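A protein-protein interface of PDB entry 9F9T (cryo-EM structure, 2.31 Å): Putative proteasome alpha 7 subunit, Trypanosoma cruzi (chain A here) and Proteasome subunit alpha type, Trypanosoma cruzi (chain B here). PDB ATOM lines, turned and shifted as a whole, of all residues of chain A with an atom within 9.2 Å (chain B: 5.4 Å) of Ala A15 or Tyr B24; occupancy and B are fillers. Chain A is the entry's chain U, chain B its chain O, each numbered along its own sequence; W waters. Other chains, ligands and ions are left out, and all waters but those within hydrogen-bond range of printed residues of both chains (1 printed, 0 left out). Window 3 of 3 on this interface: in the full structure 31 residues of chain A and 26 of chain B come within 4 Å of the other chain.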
ATOM      1  N   HIS A   6      12.919 -19.594  -1.725  1.00  0.00           N
ATOM      2  CA  HIS A   6      11.638 -20.264  -1.909  1.00  0.00           C
ATOM      3  C   HIS A   6      10.703 -19.989  -0.732  1.00  0.00           C
ATOM      4  O   HIS A   6       9.661 -20.635  -0.651  1.00  0.00           O
ATOM      5  CB  HIS A   6      11.818 -21.776  -2.116  1.00  0.00           C
ATOM      6  CG  HIS A   6      12.505 -22.440  -0.981  1.00  0.00           C
ATOM      7  ND1 HIS A   6      13.877 -22.501  -0.876  1.00  0.00           N
ATOM      8  CD2 HIS A   6      12.023 -22.990   0.137  1.00  0.00           C
ATOM      9  CE1 HIS A   6      14.204 -23.113   0.259  1.00  0.00           C
ATOM     10  NE2 HIS A   6      13.093 -23.425   0.888  1.00  0.00           N
ATOM     11  N   ASP A   7      11.063 -19.053   0.166  1.00  0.00           N
ATOM     12  CA  ASP A   7      10.309 -18.944   1.397  1.00  0.00           C
ATOM     13  C   ASP A   7       9.892 -17.520   1.691  1.00  0.00           C
ATOM     14  O   ASP A   7       9.667 -17.179   2.838  1.00  0.00           O
ATOM     15  CB  ASP A   7      11.035 -19.630   2.551  1.00  0.00           C
ATOM     16  CG  ASP A   7      12.094 -18.785   3.188  1.00  0.00           C
ATOM     17  OD1 ASP A   7      12.454 -19.090   4.368  1.00  0.00           O
ATOM     18  OD2 ASP A   7      12.555 -17.837   2.491  1.00  0.00           O
ATOM     19  N   ILE A  12       4.194 -19.919  -3.736  1.00  0.00           N
ATOM     20  CA  ILE A  12       5.317 -20.678  -4.280  1.00  0.00           C
ATOM     21  C   ILE A  12       5.450 -22.030  -3.583  1.00  0.00           C
ATOM     22  O   ILE A  12       5.656 -22.069  -2.372  1.00  0.00           O
ATOM     23  CB  ILE A  12       6.611 -19.887  -4.011  1.00  0.00           C
ATOM     24  CG1 ILE A  12       6.809 -18.733  -4.975  1.00  0.00           C
ATOM     25  CG2 ILE A  12       7.855 -20.759  -4.058  1.00  0.00           C
ATOM     26  CD1 ILE A  12       8.054 -17.893  -4.634  1.00  0.00           C
ATOM     27  N   PHE A  13       5.446 -23.160  -4.292  1.00  0.00           N
ATOM     28  CA  PHE A  13       5.879 -24.327  -3.550  1.00  0.00           C
ATOM     29  C   PHE A  13       7.386 -24.315  -3.452  1.00  0.00           C
ATOM     30  O   PHE A  13       8.082 -23.835  -4.348  1.00  0.00           O
ATOM     31  CB  PHE A  13       5.445 -25.666  -4.129  1.00  0.00           C
ATOM     32  CG  PHE A  13       3.989 -25.970  -3.941  1.00  0.00           C
ATOM     33  CD1 PHE A  13       3.542 -26.505  -2.740  1.00  0.00           C
ATOM     34  CD2 PHE A  13       3.070 -25.577  -4.897  1.00  0.00           C
ATOM     35  CE1 PHE A  13       2.204 -26.757  -2.531  1.00  0.00           C
ATOM     36  CE2 PHE A  13       1.713 -25.806  -4.680  1.00  0.00           C
ATOM     37  CZ  PHE A  13       1.293 -26.421  -3.519  1.00  0.00           C
ATOM     38  N   SER A  14       7.840 -24.943  -2.384  1.00  0.00           N
ATOM     39  CA  SER A  14       9.203 -25.384  -2.247  1.00  0.00           C
ATOM     40  C   SER A  14       9.390 -26.667  -3.047  1.00  0.00           C
ATOM     41  O   SER A  14       8.398 -27.269  -3.449  1.00  0.00           O
ATOM     42  CB  SER A  14       9.467 -25.672  -0.817  1.00  0.00           C
ATOM     43  OG  SER A  14       9.328 -27.063  -0.551  1.00  0.00           O
ATOM     44  N   ALA A  15      10.615 -27.201  -3.125  1.00  0.00           N
ATOM     45  CA  ALA A  15      10.816 -28.354  -3.998  1.00  0.00           C
ATOM     46  C   ALA A  15      10.251 -29.651  -3.400  1.00  0.00           C
ATOM     47  O   ALA A  15      10.123 -30.655  -4.090  1.00  0.00           O
ATOM     48  CB  ALA A  15      12.244 -28.491  -4.404  1.00  0.00           C
ATOM     49  N   ASP A  16       9.863 -29.622  -2.135  1.00  0.00           N
ATOM     50  CA  ASP A  16       9.415 -30.808  -1.422  1.00  0.00           C
ATOM     51  C   ASP A  16       7.892 -30.828  -1.366  1.00  0.00           C
ATOM     52  O   ASP A  16       7.313 -31.683  -0.739  1.00  0.00           O
ATOM     53  CB  ASP A  16      10.001 -30.772  -0.013  1.00  0.00           C
ATOM     54  CG  ASP A  16      10.826 -32.009   0.238  1.00  0.00           C
ATOM     55  OD1 ASP A  16      10.196 -33.096   0.397  1.00  0.00           O
ATOM     56  OD2 ASP A  16      12.083 -31.899   0.200  1.00  0.00           O
ATOM     57  N   GLY A  17       7.278 -29.785  -1.913  1.00  0.00           N
ATOM     58  CA  GLY A  17       5.849 -29.599  -1.901  1.00  0.00           C
ATOM     59  C   GLY A  17       5.315 -28.899  -0.650  1.00  0.00           C
ATOM     60  O   GLY A  17       4.160 -29.090  -0.286  1.00  0.00           O
ATOM     61  N   ARG A  18       6.147 -28.108   0.023  1.00  0.00           N
ATOM     62  CA  ARG A  18       5.740 -27.410   1.226  1.00  0.00           C
ATOM     63  C   ARG A  18       5.463 -25.966   0.889  1.00  0.00           C
ATOM     64  O   ARG A  18       5.872 -25.530  -0.157  1.00  0.00           O
ATOM     65  CB  ARG A  18       6.845 -27.577   2.245  1.00  0.00           C
ATOM     66  CG  ARG A  18       6.876 -29.018   2.685  1.00  0.00           C
ATOM     67  CD  ARG A  18       8.065 -29.317   3.507  1.00  0.00           C
ATOM     68  NE  ARG A  18       8.143 -28.460   4.675  1.00  0.00           N
ATOM     69  CZ  ARG A  18       9.237 -28.366   5.433  1.00  0.00           C
ATOM     70  NH1 ARG A  18       9.202 -27.630   6.528  1.00  0.00           N
ATOM     71  NH2 ARG A  18      10.348 -29.003   5.065  1.00  0.00           N
ATOM     72  N   VAL A  19       4.711 -25.266   1.731  1.00  0.00           N
ATOM     73  CA  VAL A  19       4.508 -23.838   1.548  1.00  0.00           C
ATOM     74  C   VAL A  19       5.002 -23.165   2.815  1.00  0.00           C
ATOM     75  O   VAL A  19       4.261 -23.163   3.794  1.00  0.00           O
ATOM     76  CB  VAL A  19       3.034 -23.458   1.335  1.00  0.00           C
ATOM     77  CG1 VAL A  19       2.902 -21.964   1.084  1.00  0.00           C
ATOM     78  CG2 VAL A  19       2.341 -24.239   0.225  1.00  0.00           C
ATOM     79  N   PHE A  20       6.226 -22.654   2.830  1.00  0.00           N
ATOM     80  CA  PHE A  20       6.898 -22.268   4.063  1.00  0.00           C
ATOM     81  C   PHE A  20       6.294 -21.007   4.707  1.00  0.00           C
ATOM     82  O   PHE A  20       6.173 -20.922   5.926  1.00  0.00           O
ATOM     83  CB  PHE A  20       8.375 -22.025   3.778  1.00  0.00           C
ATOM     84  CG  PHE A  20       9.225 -23.266   3.761  1.00  0.00           C
ATOM     85  CD1 PHE A  20       9.685 -23.824   4.919  1.00  0.00           C
ATOM     86  CD2 PHE A  20       9.636 -23.840   2.587  1.00  0.00           C
ATOM     87  CE1 PHE A  20      10.557 -24.904   4.901  1.00  0.00           C
ATOM     88  CE2 PHE A  20      10.456 -24.955   2.576  1.00  0.00           C
ATOM     89  CZ  PHE A  20      10.908 -25.490   3.730  1.00  0.00           C
ATOM     90  N   LYS B   8      12.425 -21.346 -10.786  1.00  0.00           N
ATOM     91  CA  LYS B   8      11.995 -22.237  -9.724  1.00  0.00           C
ATOM     92  C   LYS B   8      10.914 -21.555  -8.907  1.00  0.00           C
ATOM     93  O   LYS B   8      10.207 -22.217  -8.175  1.00  0.00           O
ATOM     94  CB  LYS B   8      13.181 -22.720  -8.892  1.00  0.00           C
ATOM     95  CG  LYS B   8      14.049 -23.760  -9.592  1.00  0.00           C
ATOM     96  CD  LYS B   8      14.980 -24.472  -8.619  1.00  0.00           C
ATOM     97  CE  LYS B   8      15.731 -25.643  -9.225  1.00  0.00           C
ATOM     98  NZ  LYS B   8      16.734 -25.206 -10.227  1.00  0.00           N
ATOM     99  N   TYR B  20       8.536 -25.787 -13.248  1.00  0.00           N
ATOM    100  CA  TYR B  20       8.991 -26.336 -11.967  1.00  0.00           C
ATOM    101  C   TYR B  20       7.898 -26.336 -10.882  1.00  0.00           C
ATOM    102  O   TYR B  20       7.831 -27.244 -10.082  1.00  0.00           O
ATOM    103  CB  TYR B  20      10.269 -25.594 -11.562  1.00  0.00           C
ATOM    104  CG  TYR B  20      11.526 -26.251 -12.118  1.00  0.00           C
ATOM    105  CD1 TYR B  20      11.764 -27.603 -11.901  1.00  0.00           C
ATOM    106  CD2 TYR B  20      12.453 -25.535 -12.888  1.00  0.00           C
ATOM    107  CE1 TYR B  20      12.893 -28.230 -12.412  1.00  0.00           C
ATOM    108  CE2 TYR B  20      13.590 -26.151 -13.392  1.00  0.00           C
ATOM    109  CZ  TYR B  20      13.804 -27.502 -13.157  1.00  0.00           C
ATOM    110  OH  TYR B  20      14.893 -28.152 -13.652  1.00  0.00           O
ATOM    111  N   GLN B  21       7.023 -25.322 -10.900  1.00  0.00           N
ATOM    112  CA  GLN B  21       5.996 -25.156  -9.898  1.00  0.00           C
ATOM    113  C   GLN B  21       4.961 -26.288 -10.014  1.00  0.00           C
ATOM    114  O   GLN B  21       4.471 -26.797  -9.013  1.00  0.00           O
ATOM    115  CB  GLN B  21       5.398 -23.745 -10.005  1.00  0.00           C
ATOM    116  CG  GLN B  21       6.185 -22.702  -9.200  1.00  0.00           C
ATOM    117  CD  GLN B  21       6.308 -23.065  -7.745  1.00  0.00           C
ATOM    118  OE1 GLN B  21       5.295 -23.335  -7.090  1.00  0.00           O
ATOM    119  NE2 GLN B  21       7.535 -23.110  -7.235  1.00  0.00           N
ATOM    120  N   VAL B  22       4.705 -26.714 -11.253  1.00  0.00           N
ATOM    121  CA  VAL B  22       3.924 -27.883 -11.559  1.00  0.00           C
ATOM    122  C   VAL B  22       4.601 -29.103 -10.970  1.00  0.00           C
ATOM    123  O   VAL B  22       3.970 -29.805 -10.185  1.00  0.00           O
ATOM    124  CB  VAL B  22       3.634 -28.054 -13.064  1.00  0.00           C
ATOM    125  CG1 VAL B  22       2.762 -29.273 -13.294  1.00  0.00           C
ATOM    126  CG2 VAL B  22       2.969 -26.826 -13.667  1.00  0.00           C
ATOM    127  N   GLU B  23       5.878 -29.324 -11.216  1.00  0.00           N
ATOM    128  CA  GLU B  23       6.453 -30.519 -10.634  1.00  0.00           C
ATOM    129  C   GLU B  23       6.380 -30.509  -9.121  1.00  0.00           C
ATOM    130  O   GLU B  23       6.327 -31.561  -8.517  1.00  0.00           O
ATOM    131  CB  GLU B  23       7.913 -30.685 -11.002  1.00  0.00           C
ATOM    132  CG  GLU B  23       8.136 -30.883 -12.499  1.00  0.00           C
ATOM    133  CD  GLU B  23       9.606 -31.126 -12.835  1.00  0.00           C
ATOM    134  OE1 GLU B  23      10.436 -31.233 -11.870  1.00  0.00           O
ATOM    135  OE2 GLU B  23       9.936 -31.183 -14.049  1.00  0.00           O
ATOM    136  N   TYR B  24       6.485 -29.344  -8.487  1.00  0.00           N
ATOM    137  CA  TYR B  24       6.538 -29.315  -7.024  1.00  0.00           C
ATOM    138  C   TYR B  24       5.157 -29.469  -6.384  1.00  0.00           C
ATOM    139  O   TYR B  24       5.045 -30.010  -5.319  1.00  0.00           O
ATOM    140  CB  TYR B  24       7.145 -27.978  -6.569  1.00  0.00           C
ATOM    141  CG  TYR B  24       8.616 -27.779  -6.905  1.00  0.00           C
ATOM    142  CD1 TYR B  24       9.425 -28.841  -7.313  1.00  0.00           C
ATOM    143  CD2 TYR B  24       9.136 -26.489  -6.957  1.00  0.00           C
ATOM    144  CE1 TYR B  24      10.742 -28.629  -7.682  1.00  0.00           C
ATOM    145  CE2 TYR B  24      10.463 -26.270  -7.311  1.00  0.00           C
ATOM    146  CZ  TYR B  24      11.261 -27.342  -7.665  1.00  0.00           C
ATOM    147  OH  TYR B  24      12.559 -27.069  -7.968  1.00  0.00           O
ATOM    148  N   ALA B  25       4.149 -28.903  -7.040  1.00  0.00           N
ATOM    149  CA  ALA B  25       2.747 -29.145  -6.760  1.00  0.00           C
ATOM    150  C   ALA B  25       2.438 -30.633  -6.811  1.00  0.00           C
ATOM    151  O   ALA B  25       1.648 -31.074  -6.008  1.00  0.00           O
ATOM    152  CB  ALA B  25       1.832 -28.329  -7.691  1.00  0.00           C
ATOM    153  N   PHE B  26       3.035 -31.398  -7.711  1.00  0.00           N
ATOM    154  CA  PHE B  26       2.892 -32.846  -7.684  1.00  0.00           C
ATOM    155  C   PHE B  26       3.527 -33.432  -6.456  1.00  0.00           C
ATOM    156  O   PHE B  26       3.029 -34.421  -5.992  1.00  0.00           O
ATOM    157  CB  PHE B  26       3.551 -33.569  -8.864  1.00  0.00           C
ATOM    158  CG  PHE B  26       2.626 -33.803 -10.022  1.00  0.00           C
ATOM    159  CD1 PHE B  26       1.734 -34.869  -9.999  1.00  0.00           C
ATOM    160  CD2 PHE B  26       2.532 -32.886 -11.038  1.00  0.00           C
ATOM    161  CE1 PHE B  26       0.826 -35.068 -11.035  1.00  0.00           C
ATOM    162  CE2 PHE B  26       1.654 -33.089 -12.098  1.00  0.00           C
ATOM    163  CZ  PHE B  26       0.798 -34.186 -12.096  1.00  0.00           C
ATOM    164  N   LYS B  27       4.579 -32.846  -5.909  1.00  0.00           N
ATOM    165  CA  LYS B  27       5.144 -33.388  -4.681  1.00  0.00           C
ATOM    166  C   LYS B  27       4.250 -33.101  -3.472  1.00  0.00           C
ATOM    167  O   LYS B  27       4.217 -33.863  -2.528  1.00  0.00           O
ATOM    168  CB  LYS B  27       6.529 -32.804  -4.408  1.00  0.00           C
ATOM    169  CG  LYS B  27       7.610 -33.165  -5.410  1.00  0.00           C
ATOM    170  CD  LYS B  27       7.822 -34.643  -5.539  1.00  0.00           C
ATOM    171  CE  LYS B  27       8.666 -35.212  -4.419  1.00  0.00           C
ATOM    172  NZ  LYS B  27      10.101 -34.896  -4.648  1.00  0.00           N
ATOM    173  N   ALA B  28       3.544 -31.969  -3.493  1.00  0.00           N
ATOM    174  CA  ALA B  28       2.598 -31.637  -2.447  1.00  0.00           C
ATOM    175  C   ALA B  28       1.609 -32.777  -2.245  1.00  0.00           C
ATOM    176  O   ALA B  28       1.170 -33.007  -1.124  1.00  0.00           O
ATOM    177  CB  ALA B  28       1.897 -30.346  -2.806  1.00  0.00           C
HETATM  178  O   HOH W   1      10.833 -22.929  -5.368  1.00  0.00           O
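Water W1 lies within hydrogen-bond range of O of Lys B8 (3.0 Å) and O of Phe A13 (3.1 Å).
Printed residues of chain A that touch a printed residue of chain B: Ile A12, Phe A13, Ser A14, Ala A15, Asp A16 and Gly A17. Hydrophobic or aromatic side chains of chain A that line the printed part of chain B: Ile A12, Phe A13 and Ala A15. Among the printed residues, no Asp or Glu carboxylate lies within 4 Å of a Lys or Arg side-chain nitrogen of the other chain.
Printed residues of chain B within 4 Å of Ile A12: Gln B21 (3.7 Å). Of the printed residues of chain B, Ser A14 touches Tyr B24. Of the printed residues of chain B, Asp A16 touches Lys B27 (3.9 Å). Of the printed residues of chain B, Gly A17 touches Tyr B24 (3.5 Å), Lys B27 (3.99 Å) and Ala B28 (3.6 Å). Phe A20 touches none of the printed residues of chain B. Printed residues of chain A within 4 Å of Tyr B24: Phe A13 (3.8 Å), Ser A14 (3.4 Å), Ala A15 (3.6 Å) and Gly A17 (3.5 Å). Ala B25 touches just one residue of chain A: Phe A13. Of the printed residues of chain A, Ala B28 touches Phe A13 and Gly A17.
The backbone carbonyl oxygen (O) of Lys B8 sits at hydrogen-bond distance from the side-chain amide nitrogen (NE2) of Gln B21 (3.0 Å). OG of Ser A14 lies within hydrogen-bond range of N of Asp A16. OG of Ser A14 is in hydrogen-bond range of N of Arg A18 (3.4 Å).
The side-chain amide oxygen (OE1) of Gln B21 is in hydrogen-bond range of the backbone NH (N) of Phe A13 (2.8 Å).
Ile A12 touches Gln B21 (C to OE1, 3.7 Å). Tyr B24 touches Phe A13 (CB to CB, 3.8 Å). Ala B25 touches Phe A13 (CB to CE2, 3.9 Å). Phe A13 touches Ala B28 (CE1 to CB, 3.6 Å). Tyr B24 touches Ser A14. Ala A15 touches Tyr B24. Ala A15 touches Lys B27. Lys B27 touches Asp A16. Gly A17 touches Tyr B24 (CA to O, 3.5 Å). Gly A17 touches Lys B27.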
